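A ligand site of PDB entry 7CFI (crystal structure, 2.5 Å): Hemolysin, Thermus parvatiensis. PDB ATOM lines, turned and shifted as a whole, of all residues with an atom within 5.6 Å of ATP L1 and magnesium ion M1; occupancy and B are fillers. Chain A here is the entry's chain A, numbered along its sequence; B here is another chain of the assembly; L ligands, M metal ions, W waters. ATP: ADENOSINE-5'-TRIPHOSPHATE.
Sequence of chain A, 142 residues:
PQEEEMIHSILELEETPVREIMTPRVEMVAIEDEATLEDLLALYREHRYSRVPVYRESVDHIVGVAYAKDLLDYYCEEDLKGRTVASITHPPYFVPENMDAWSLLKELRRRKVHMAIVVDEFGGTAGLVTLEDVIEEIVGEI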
ATOM      1  N   MET A  22      28.661 -20.276  -4.769  1.00  0.00           N
ATOM      2  CA  MET A  22      28.059 -21.407  -4.088  1.00  0.00           C
ATOM      3  C   MET A  22      27.960 -21.168  -2.579  1.00  0.00           C
ATOM      4  O   MET A  22      28.527 -20.217  -2.031  1.00  0.00           O
ATOM      5  CB  MET A  22      28.897 -22.662  -4.334  1.00  0.00           C
ATOM      6  CG  MET A  22      30.314 -22.535  -3.784  1.00  0.00           C
ATOM      7  SD  MET A  22      31.318 -24.027  -3.872  1.00  0.00           S
ATOM      8  CE  MET A  22      32.863 -23.406  -3.182  1.00  0.00           C
ATOM      9  N   THR A  23      27.219 -22.055  -1.914  1.00  0.00           N
ATOM     10  CA  THR A  23      27.266 -22.168  -0.468  1.00  0.00           C
ATOM     11  C   THR A  23      28.268 -23.245  -0.092  1.00  0.00           C
ATOM     12  O   THR A  23      28.090 -24.401  -0.475  1.00  0.00           O
ATOM     13  CB  THR A  23      25.893 -22.517   0.090  1.00  0.00           C
ATOM     14  OG1 THR A  23      25.032 -21.365   0.036  1.00  0.00           O
ATOM     15  CG2 THR A  23      26.009 -22.987   1.540  1.00  0.00           C
ATOM     16  N   GLU A  27      28.911 -24.881   5.521  1.00  0.00           N
ATOM     17  CA  GLU A  27      27.664 -24.192   5.831  1.00  0.00           C
ATOM     18  C   GLU A  27      26.464 -24.938   5.276  1.00  0.00           C
ATOM     19  O   GLU A  27      25.333 -24.433   5.359  1.00  0.00           O
ATOM     20  CB  GLU A  27      27.724 -22.765   5.297  1.00  0.00           C
ATOM     21  CG  GLU A  27      28.746 -21.912   6.030  1.00  0.00           C
ATOM     22  CD  GLU A  27      28.871 -20.509   5.471  1.00  0.00           C
ATOM     23  OE1 GLU A  27      29.121 -19.573   6.267  1.00  0.00           O
ATOM     24  OE2 GLU A  27      28.734 -20.334   4.247  1.00  0.00           O
ATOM     25  N   MET A  28      26.664 -26.133   4.725  1.00  0.00           N
ATOM     26  CA  MET A  28      25.565 -26.967   4.259  1.00  0.00           C
ATOM     27  C   MET A  28      24.812 -27.592   5.421  1.00  0.00           C
ATOM     28  O   MET A  28      25.410 -28.048   6.400  1.00  0.00           O
ATOM     29  CB  MET A  28      26.089 -28.085   3.372  1.00  0.00           C
ATOM     30  CG  MET A  28      26.613 -27.704   2.038  1.00  0.00           C
ATOM     31  SD  MET A  28      27.377 -29.189   1.328  1.00  0.00           S
ATOM     32  CE  MET A  28      25.978 -30.275   1.070  1.00  0.00           C
ATOM     33  N   VAL A  29      23.490 -27.659   5.269  1.00  0.00           N
ATOM     34  CA  VAL A  29      22.637 -28.479   6.118  1.00  0.00           C
ATOM     35  C   VAL A  29      22.287 -29.732   5.345  1.00  0.00           C
ATOM     36  O   VAL A  29      21.606 -29.676   4.324  1.00  0.00           O
ATOM     37  CB  VAL A  29      21.379 -27.712   6.536  1.00  0.00           C
ATOM     38  CG1 VAL A  29      20.406 -28.627   7.252  1.00  0.00           C
ATOM     39  CG2 VAL A  29      21.746 -26.506   7.396  1.00  0.00           C
ATOM     40  N   ALA A  30      22.761 -30.881   5.827  1.00  0.00           N
ATOM     41  CA  ALA A  30      22.586 -32.155   5.131  1.00  0.00           C
ATOM     42  C   ALA A  30      22.119 -33.216   6.110  1.00  0.00           C
ATOM     43  O   ALA A  30      22.074 -32.987   7.331  1.00  0.00           O
ATOM     44  CB  ALA A  30      23.880 -32.587   4.428  1.00  0.00           C
ATOM     45  N   ARG A  48      14.920 -24.858   8.169  1.00  0.00           N
ATOM     46  CA  ARG A  48      13.935 -24.292   7.238  1.00  0.00           C
ATOM     47  C   ARG A  48      14.379 -24.320   5.782  1.00  0.00           C
ATOM     48  O   ARG A  48      13.781 -23.619   4.951  1.00  0.00           O
ATOM     49  CB  ARG A  48      13.550 -22.859   7.605  1.00  0.00           C
ATOM     50  CG  ARG A  48      13.008 -22.719   9.026  1.00  0.00           C
ATOM     51  CD  ARG A  48      12.113 -23.901   9.358  1.00  0.00           C
ATOM     52  NE  ARG A  48      11.353 -23.720  10.588  1.00  0.00           N
ATOM     53  CZ  ARG A  48      10.141 -23.182  10.635  1.00  0.00           C
ATOM     54  NH1 ARG A  48       9.551 -22.788   9.516  1.00  0.00           N
ATOM     55  NH2 ARG A  48       9.516 -23.060  11.794  1.00  0.00           N
ATOM     56  N   TYR A  49      15.380 -25.114   5.431  1.00  0.00           N
ATOM     57  CA  TYR A  49      15.741 -25.258   4.025  1.00  0.00           C
ATOM     58  C   TYR A  49      14.792 -26.249   3.348  1.00  0.00           C
ATOM     59  O   TYR A  49      14.408 -27.269   3.925  1.00  0.00           O
ATOM     60  CB  TYR A  49      17.190 -25.727   3.878  1.00  0.00           C
ATOM     61  CG  TYR A  49      18.184 -24.633   4.185  1.00  0.00           C
ATOM     62  CD1 TYR A  49      18.370 -23.570   3.312  1.00  0.00           C
ATOM     63  CD2 TYR A  49      18.957 -24.665   5.344  1.00  0.00           C
ATOM     64  CE1 TYR A  49      19.281 -22.559   3.581  1.00  0.00           C
ATOM     65  CE2 TYR A  49      19.876 -23.667   5.622  1.00  0.00           C
ATOM     66  CZ  TYR A  49      20.030 -22.620   4.744  1.00  0.00           C
ATOM     67  OH  TYR A  49      20.941 -21.623   5.016  1.00  0.00           O
ATOM     68  N   SER A  50      14.398 -25.920   2.115  1.00  0.00           N
ATOM     69  CA  SER A  50      13.449 -26.756   1.385  1.00  0.00           C
ATOM     70  C   SER A  50      14.123 -27.974   0.770  1.00  0.00           C
ATOM     71  O   SER A  50      13.501 -29.034   0.670  1.00  0.00           O
ATOM     72  CB  SER A  50      12.748 -25.935   0.299  1.00  0.00           C
ATOM     73  OG  SER A  50      11.957 -24.905   0.863  1.00  0.00           O
ATOM     74  N   ARG A  51      15.390 -27.844   0.364  1.00  0.00           N
ATOM     75  CA  ARG A  51      16.143 -28.912  -0.273  1.00  0.00           C
ATOM     76  C   ARG A  51      17.379 -29.207   0.555  1.00  0.00           C
ATOM     77  O   ARG A  51      18.153 -28.293   0.873  1.00  0.00           O
ATOM     78  CB  ARG A  51      16.503 -28.542  -1.706  1.00  0.00           C
ATOM     79  CG  ARG A  51      15.314 -28.487  -2.662  1.00  0.00           C
ATOM     80  CD  ARG A  51      15.724 -28.211  -4.103  1.00  0.00           C
ATOM     81  NE  ARG A  51      14.622 -27.731  -4.932  1.00  0.00           N
ATOM     82  CZ  ARG A  51      13.949 -26.594  -4.733  1.00  0.00           C
ATOM     83  NH1 ARG A  51      14.278 -25.780  -3.730  1.00  0.00           N
ATOM     84  NH2 ARG A  51      12.964 -26.257  -5.543  1.00  0.00           N
ATOM     85  N   VAL A  52      17.576 -30.484   0.881  1.00  0.00           N
ATOM     86  CA  VAL A  52      18.660 -30.920   1.753  1.00  0.00           C
ATOM     87  C   VAL A  52      19.468 -31.974   1.030  1.00  0.00           C
ATOM     88  O   VAL A  52      18.926 -32.995   0.598  1.00  0.00           O
ATOM     89  CB  VAL A  52      18.116 -31.481   3.091  1.00  0.00           C
ATOM     90  CG1 VAL A  52      19.250 -32.064   3.907  1.00  0.00           C
ATOM     91  CG2 VAL A  52      17.401 -30.385   3.867  1.00  0.00           C
ATOM     92  N   PRO A  53      20.790 -31.795   0.866  1.00  0.00           N
ATOM     93  CA  PRO A  53      21.611 -32.859   0.305  1.00  0.00           C
ATOM     94  C   PRO A  53      21.667 -34.060   1.235  1.00  0.00           C
ATOM     95  O   PRO A  53      21.542 -33.943   2.453  1.00  0.00           O
ATOM     96  CB  PRO A  53      22.997 -32.200   0.154  1.00  0.00           C
ATOM     97  CG  PRO A  53      22.707 -30.727   0.185  1.00  0.00           C
ATOM     98  CD  PRO A  53      21.552 -30.565   1.105  1.00  0.00           C
ATOM     99  N   HIS A 114      16.721 -27.633  -9.263  1.00  0.00           N
ATOM    100  CA  HIS A 114      16.935 -26.346  -8.620  1.00  0.00           C
ATOM    101  C   HIS A 114      18.259 -26.269  -7.862  1.00  0.00           C
ATOM    102  O   HIS A 114      18.730 -25.159  -7.588  1.00  0.00           O
ATOM    103  CB  HIS A 114      15.781 -26.038  -7.657  1.00  0.00           C
ATOM    104  CG  HIS A 114      15.793 -24.637  -7.129  1.00  0.00           C
ATOM    105  ND1 HIS A 114      16.859 -24.107  -6.437  1.00  0.00           N
ATOM    106  CD2 HIS A 114      14.852 -23.662  -7.185  1.00  0.00           C
ATOM    107  CE1 HIS A 114      16.585 -22.862  -6.096  1.00  0.00           C
ATOM    108  NE2 HIS A 114      15.370 -22.563  -6.534  1.00  0.00           N
ATOM    109  N   MET A 115      18.855 -27.408  -7.501  1.00  0.00           N
ATOM    110  CA  MET A 115      20.062 -27.433  -6.686  1.00  0.00           C
ATOM    111  C   MET A 115      21.077 -28.372  -7.308  1.00  0.00           C
ATOM    112  O   MET A 115      20.752 -29.506  -7.660  1.00  0.00           O
ATOM    113  CB  MET A 115      19.742 -27.866  -5.254  1.00  0.00           C
ATOM    114  CG  MET A 115      20.938 -28.460  -4.513  1.00  0.00           C
ATOM    115  SD  MET A 115      20.623 -28.774  -2.763  1.00  0.00           S
ATOM    116  CE  MET A 115      19.918 -27.211  -2.258  1.00  0.00           C
ATOM    117  N   LEU A 128      27.221 -26.491  -2.332  1.00  0.00           N
ATOM    118  CA  LEU A 128      26.021 -26.556  -3.165  1.00  0.00           C
ATOM    119  C   LEU A 128      25.806 -25.190  -3.810  1.00  0.00           C
ATOM    120  O   LEU A 128      26.353 -24.177  -3.382  1.00  0.00           O
ATOM    121  CB  LEU A 128      24.768 -26.960  -2.358  1.00  0.00           C
ATOM    122  CG  LEU A 128      24.360 -26.133  -1.139  1.00  0.00           C
ATOM    123  CD1 LEU A 128      23.482 -24.934  -1.505  1.00  0.00           C
ATOM    124  CD2 LEU A 128      23.665 -27.004  -0.103  1.00  0.00           C
ATOM    125  N   VAL A 129      24.955 -25.186  -4.835  1.00  0.00           N
ATOM    126  CA  VAL A 129      24.575 -23.959  -5.531  1.00  0.00           C
ATOM    127  C   VAL A 129      23.184 -24.170  -6.110  1.00  0.00           C
ATOM    128  O   VAL A 129      22.868 -25.225  -6.652  1.00  0.00           O
ATOM    129  CB  VAL A 129      25.615 -23.582  -6.616  1.00  0.00           C
ATOM    130  CG1 VAL A 129      25.560 -24.548  -7.792  1.00  0.00           C
ATOM    131  CG2 VAL A 129      25.432 -22.150  -7.076  1.00  0.00           C
ATOM    132  N   THR A 130      22.332 -23.162  -5.947  1.00  0.00           N
ATOM    133  CA  THR A 130      20.952 -23.247  -6.360  1.00  0.00           C
ATOM    134  C   THR A 130      20.676 -22.238  -7.454  1.00  0.00           C
ATOM    135  O   THR A 130      21.474 -21.333  -7.711  1.00  0.00           O
ATOM    136  CB  THR A 130      19.996 -22.999  -5.193  1.00  0.00           C
ATOM    137  OG1 THR A 130      20.143 -21.647  -4.756  1.00  0.00           O
ATOM    138  CG2 THR A 130      20.336 -23.933  -4.020  1.00  0.00           C
ATOM    139  N   LEU A 131      19.513 -22.402  -8.100  1.00  0.00           N
ATOM    140  CA  LEU A 131      19.084 -21.423  -9.095  1.00  0.00           C
ATOM    141  C   LEU A 131      18.984 -20.012  -8.494  1.00  0.00           C
ATOM    142  O   LEU A 131      19.234 -19.027  -9.188  1.00  0.00           O
ATOM    143  CB  LEU A 131      17.757 -21.842  -9.717  1.00  0.00           C
ATOM    144  N   GLU A 132      18.613 -19.914  -7.210  1.00  0.00           N
ATOM    145  CA  GLU A 132      18.536 -18.591  -6.585  1.00  0.00           C
ATOM    146  C   GLU A 132      19.911 -17.928  -6.531  1.00  0.00           C
ATOM    147  O   GLU A 132      20.029 -16.715  -6.730  1.00  0.00           O
ATOM    148  CB  GLU A 132      17.926 -18.675  -5.186  1.00  0.00           C
ATOM    149  CG  GLU A 132      17.622 -17.276  -4.605  1.00  0.00           C
ATOM    150  CD  GLU A 132      17.176 -17.285  -3.154  1.00  0.00           C
ATOM    151  OE1 GLU A 132      15.952 -17.348  -2.898  1.00  0.00           O
ATOM    152  OE2 GLU A 132      18.041 -17.255  -2.252  1.00  0.00           O
ATOM    153  N   ASP A 133      20.959 -18.699  -6.222  1.00  0.00           N
ATOM    154  CA  ASP A 133      22.306 -18.127  -6.223  1.00  0.00           C
ATOM    155  C   ASP A 133      22.648 -17.567  -7.600  1.00  0.00           C
ATOM    156  O   ASP A 133      23.229 -16.485  -7.713  1.00  0.00           O
ATOM    157  CB  ASP A 133      23.335 -19.164  -5.794  1.00  0.00           C
ATOM    158  CG  ASP A 133      23.122 -19.608  -4.364  1.00  0.00           C
ATOM    159  OD1 ASP A 133      23.071 -18.732  -3.486  1.00  0.00           O
ATOM    160  OD2 ASP A 133      23.015 -20.834  -4.126  1.00  0.00           O
ATOM    161  N   GLU A 136      20.570 -14.363  -8.163  1.00  0.00           N
ATOM    162  CA  GLU A 136      21.026 -13.198  -7.418  1.00  0.00           C
ATOM    163  C   GLU A 136      22.235 -12.516  -8.047  1.00  0.00           C
ATOM    164  O   GLU A 136      22.442 -11.336  -7.802  1.00  0.00           O
ATOM    165  CB  GLU A 136      21.355 -13.583  -5.979  1.00  0.00           C
ATOM    166  CG  GLU A 136      20.131 -13.901  -5.179  1.00  0.00           C
ATOM    167  CD  GLU A 136      20.472 -14.416  -3.821  1.00  0.00           C
ATOM    168  OE1 GLU A 136      21.580 -14.095  -3.321  1.00  0.00           O
ATOM    169  OE2 GLU A 136      19.634 -15.142  -3.236  1.00  0.00           O
ATOM    170  N   GLU A 141      19.912  -9.724  -4.641  1.00  0.00           N
ATOM    171  CA  GLU A 141      19.846 -10.613  -3.491  1.00  0.00           C
ATOM    172  C   GLU A 141      18.399 -10.777  -3.081  1.00  0.00           C
ATOM    173  O   GLU A 141      17.674  -9.787  -2.957  1.00  0.00           O
ATOM    174  CB  GLU A 141      20.686 -10.079  -2.328  1.00  0.00           C
ATOM    175  N   ILE A 142      17.976 -12.024  -2.882  1.00  0.00           N
ATOM    176  CA  ILE A 142      16.568 -12.312  -2.634  1.00  0.00           C
ATOM    177  C   ILE A 142      16.383 -13.002  -1.290  1.00  0.00           C
ATOM    178  O   ILE A 142      16.815 -14.144  -1.095  1.00  0.00           O
ATOM    179  CB  ILE A 142      15.985 -13.171  -3.778  1.00  0.00           C
ATOM    180  CG1 ILE A 142      15.769 -12.304  -5.023  1.00  0.00           C
ATOM    181  CG2 ILE A 142      14.661 -13.790  -3.359  1.00  0.00           C
ATOM    182  CD1 ILE A 142      15.717 -13.097  -6.308  1.00  0.00           C
ATOM    183  N   ARG B  51       2.808 -22.234  -2.526  1.00  0.00           N
ATOM    184  CA  ARG B  51       2.140 -21.045  -2.024  1.00  0.00           C
ATOM    185  C   ARG B  51       0.721 -20.997  -2.566  1.00  0.00           C
ATOM    186  O   ARG B  51       0.522 -21.106  -3.788  1.00  0.00           O
ATOM    187  CB  ARG B  51       2.919 -19.788  -2.390  1.00  0.00           C
ATOM    188  CG  ARG B  51       4.253 -19.637  -1.663  1.00  0.00           C
ATOM    189  CD  ARG B  51       4.951 -18.315  -1.978  1.00  0.00           C
ATOM    190  NE  ARG B  51       6.381 -18.342  -1.663  1.00  0.00           N
ATOM    191  CZ  ARG B  51       7.283 -19.151  -2.225  1.00  0.00           C
ATOM    192  NH1 ARG B  51       6.916 -20.006  -3.170  1.00  0.00           N
ATOM    193  NH2 ARG B  51       8.557 -19.086  -1.852  1.00  0.00           N
HETATM  194  PG  ATP L   1      12.883 -22.381  -1.615  1.00  0.00           P
HETATM  195  O1G ATP L   1      11.921 -22.816  -0.548  1.00  0.00           O
HETATM  196  O2G ATP L   1      13.114 -20.887  -1.653  1.00  0.00           O
HETATM  197  O3G ATP L   1      12.633 -22.959  -2.981  1.00  0.00           O
HETATM  198  PB  ATP L   1      15.289 -22.489  -0.027  1.00  0.00           P
HETATM  199  O1B ATP L   1      14.944 -21.100   0.399  1.00  0.00           O
HETATM  200  O2B ATP L   1      15.401 -23.586   1.018  1.00  0.00           O
HETATM  201  O3B ATP L   1      14.327 -23.004  -1.221  1.00  0.00           O
HETATM  202  PA  ATP L   1      17.033 -21.401  -1.976  1.00  0.00           P
HETATM  203  O1A ATP L   1      16.049 -20.259  -1.908  1.00  0.00           O
HETATM  204  O2A ATP L   1      17.200 -22.144  -3.271  1.00  0.00           O
HETATM  205  O3A ATP L   1      16.707 -22.461  -0.802  1.00  0.00           O
HETATM  206  O5' ATP L   1      18.474 -20.868  -1.490  1.00  0.00           O
HETATM  207  C5' ATP L   1      18.615 -19.790  -0.577  1.00  0.00           C
HETATM  208  C4' ATP L   1      20.081 -19.747  -0.131  1.00  0.00           C
HETATM  209  O4' ATP L   1      20.334 -20.767   0.834  1.00  0.00           O
HETATM  210  C3' ATP L   1      20.998 -20.012  -1.309  1.00  0.00           C
HETATM  211  O3' ATP L   1      22.122 -19.136  -1.221  1.00  0.00           O
HETATM  212  C2' ATP L   1      21.480 -21.445  -1.137  1.00  0.00           C
HETATM  213  O2' ATP L   1      22.818 -21.600  -1.578  1.00  0.00           O
HETATM  214  C1' ATP L   1      21.342 -21.671   0.357  1.00  0.00           C
HETATM  215  N9  ATP L   1      20.925 -23.068   0.633  1.00  0.00           N
HETATM  216  C8  ATP L   1      19.966 -23.750  -0.010  1.00  0.00           C
HETATM  217  N7  ATP L   1      19.840 -24.998   0.496  1.00  0.00           N
HETATM  218  C5  ATP L   1      20.733 -25.124   1.483  1.00  0.00           C
HETATM  219  C6  ATP L   1      21.127 -26.183   2.442  1.00  0.00           C
HETATM  220  N6  ATP L   1      20.520 -27.393   2.425  1.00  0.00           N
HETATM  221  N1  ATP L   1      22.111 -25.907   3.330  1.00  0.00           N
HETATM  222  C2  ATP L   1      22.730 -24.703   3.350  1.00  0.00           C
HETATM  223  N3  ATP L   1      22.416 -23.696   2.512  1.00  0.00           N
HETATM  224  C4  ATP L   1      21.457 -23.844   1.579  1.00  0.00           C
HETATM  225  PG  ATP L   2       8.353 -23.344  -5.352  1.00  0.00           P
HETATM  226  O1G ATP L   2       8.139 -24.603  -4.556  1.00  0.00           O
HETATM  227  O2G ATP L   2       8.998 -23.588  -6.698  1.00  0.00           O
HETATM  228  O3G ATP L   2       8.999 -22.215  -4.608  1.00  0.00           O
HETATM  229  PB  ATP L   2       5.854 -23.370  -6.793  1.00  0.00           P
HETATM  230  O1B ATP L   2       6.552 -24.269  -7.773  1.00  0.00           O
HETATM  231  O2B ATP L   2       4.625 -23.883  -6.068  1.00  0.00           O
HETATM  232  O3B ATP L   2       6.884 -22.757  -5.706  1.00  0.00           O
HETATM  233  PA  ATP L   2       6.413 -21.168  -8.484  1.00  0.00           P
HETATM  234  O1A ATP L   2       7.597 -22.039  -8.865  1.00  0.00           O
HETATM  235  O2A ATP L   2       6.667 -19.838  -7.852  1.00  0.00           O
HETATM  236  O3A ATP L   2       5.409 -22.021  -7.553  1.00  0.00           O
HETATM  237  O5' ATP L   2       5.495 -20.969  -9.793  1.00  0.00           O
HETATM  238  C5' ATP L   2       5.434 -21.917 -10.837  1.00  0.00           C
HETATM  239  C4' ATP L   2       4.273 -21.535 -11.747  1.00  0.00           C
HETATM  240  O4' ATP L   2       3.027 -21.923 -11.160  1.00  0.00           O
HETATM  241  C3' ATP L   2       4.216 -20.033 -11.945  1.00  0.00           C
HETATM  242  O3' ATP L   2       3.899 -19.756 -13.309  1.00  0.00           O
HETATM  243  C2' ATP L   2       3.076 -19.554 -11.073  1.00  0.00           C
HETATM  244  O2' ATP L   2       2.379 -18.458 -11.669  1.00  0.00           O
HETATM  245  C1' ATP L   2       2.189 -20.777 -10.952  1.00  0.00           C
HETATM  246  N9  ATP L   2       1.575 -20.857  -9.612  1.00  0.00           N
HETATM  247  C8  ATP L   2       2.206 -20.639  -8.435  1.00  0.00           C
HETATM  248  N7  ATP L   2       1.353 -20.788  -7.396  1.00  0.00           N
HETATM  249  C5  ATP L   2       0.155 -21.099  -7.899  1.00  0.00           C
HETATM  250  C6  ATP L   2      -1.191 -21.399  -7.355  1.00  0.00           C
HETATM  251  N6  ATP L   2      -1.417 -21.379  -6.020  1.00  0.00           N
HETATM  252  N1  ATP L   2      -2.184 -21.688  -8.228  1.00  0.00           N
HETATM  253  C2  ATP L   2      -1.970 -21.701  -9.565  1.00  0.00           C
HETATM  254  N3  ATP L   2      -0.772 -21.446 -10.125  1.00  0.00           N
HETATM  255  C4  ATP L   2       0.305 -21.139  -9.359  1.00  0.00           C
HETATM  256 MG    MG M   1      19.241 -15.786  -1.134  1.00  0.00          MG
HETATM  257 MG    MG M   2      14.040 -18.550  -0.505  1.00  0.00          MG
HETATM  258  O   HOH W   1      17.068 -25.395   0.125  1.00  0.00           O
HETATM  259  O   HOH W   2      11.320 -20.766   0.626  1.00  0.00           O
HETATM  260  O   HOH W   3      13.611 -18.634   1.635  1.00  0.00           O
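Magnesium ion M1 is bound by the side-chain carboxylate of Glu 132 (2.2 Å) and the side-chain carboxylate of Glu 136 (2.2 Å).
Merely in contact with ATP L1: Glu 27 (3.3 Å), Met 28 (3.7 Å), Tyr 49 (3.2 Å), Pro 53 (3.6 Å), His 114 (3.0 Å), Met 115 (3.5 Å) and Leu 128 (3.4 Å). Hydrophobic or aromatic side chains that line ATP L1: Val 29, Tyr 49, Pro 53, His 114, Met 115 and Leu 128. Along chain A the residues within 4 Å of ATP L1 span positions 23 to 133. The nearest printed residue that does not touch ATP L1 is Val 52 (4.04 Å).
Water W1 lies within hydrogen-bond range of O2B of ATP L1 (2.6 Å), N of Arg 51 of chain A (3.0 Å) and N of Ser 50 (3.4 Å).
The side-chain carboxylate of Glu 132 lies close to an oxygen (O1A) of ATP L1 (3.1 Å). OD1 of Asp 133 is in hydrogen-bond range of O3' of ATP L1, at 2.5 Å. The backbone NH (N) of Ser 50 sits at hydrogen-bond distance from an oxygen (O2B) of ATP L1. OG of Ser 50 sits at hydrogen-bond distance from O1G of ATP L1. OG1 of Thr 23 sits at hydrogen-bond distance from O2' of ATP L1. N of Val 29 sits at hydrogen-bond distance from N1 of ATP L1. O of Val 29 sits at hydrogen-bond distance from N6 of ATP L1 (3.2 Å). The backbone carbonyl oxygen (O) of Arg 51 of chain A is in hydrogen-bond range of a nitrogen (N6) of ATP L1 (3.0 Å). The guanidinium group (NH1) of Arg 51 of chain A lies within salt-bridge range of an oxygen (O3G) of ATP L1 (3.4 Å). OG1 of Thr 130 lies within hydrogen-bond range of O2A of ATP L1 (3.3 Å). The backbone carbonyl oxygen (O) of Arg 51 of chain B sits at hydrogen-bond distance from a nitrogen (N6) of ATP L2 (3.0 Å). The guanidinium group (NH1) of Arg 51 of chain B lies within salt-bridge range of an oxygen (O3G) of ATP L2, at 3.4 Å.
N of Glu 132 sits close to OG1 of Thr 130 (3.4 Å). The side-chain carboxylate (OD2) of Asp 133 is in hydrogen-bond range of the backbone NH (N) of Thr 130 (3.0 Å). The backbone NH (N) of Thr 23 sits at hydrogen-bond distance from the backbone carbonyl oxygen (O) of Leu 128, at 2.7 Å. N of Leu 131 sits at hydrogen-bond distance from O of His 114.
Merely in contact with magnesium ion M1: Ile 142. Along chain A the residues within 4 Å of magnesium ion M1 span positions 132 to 142. The nearest printed residue that does not touch magnesium ion M1 is Asp 133 (5.4 Å).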
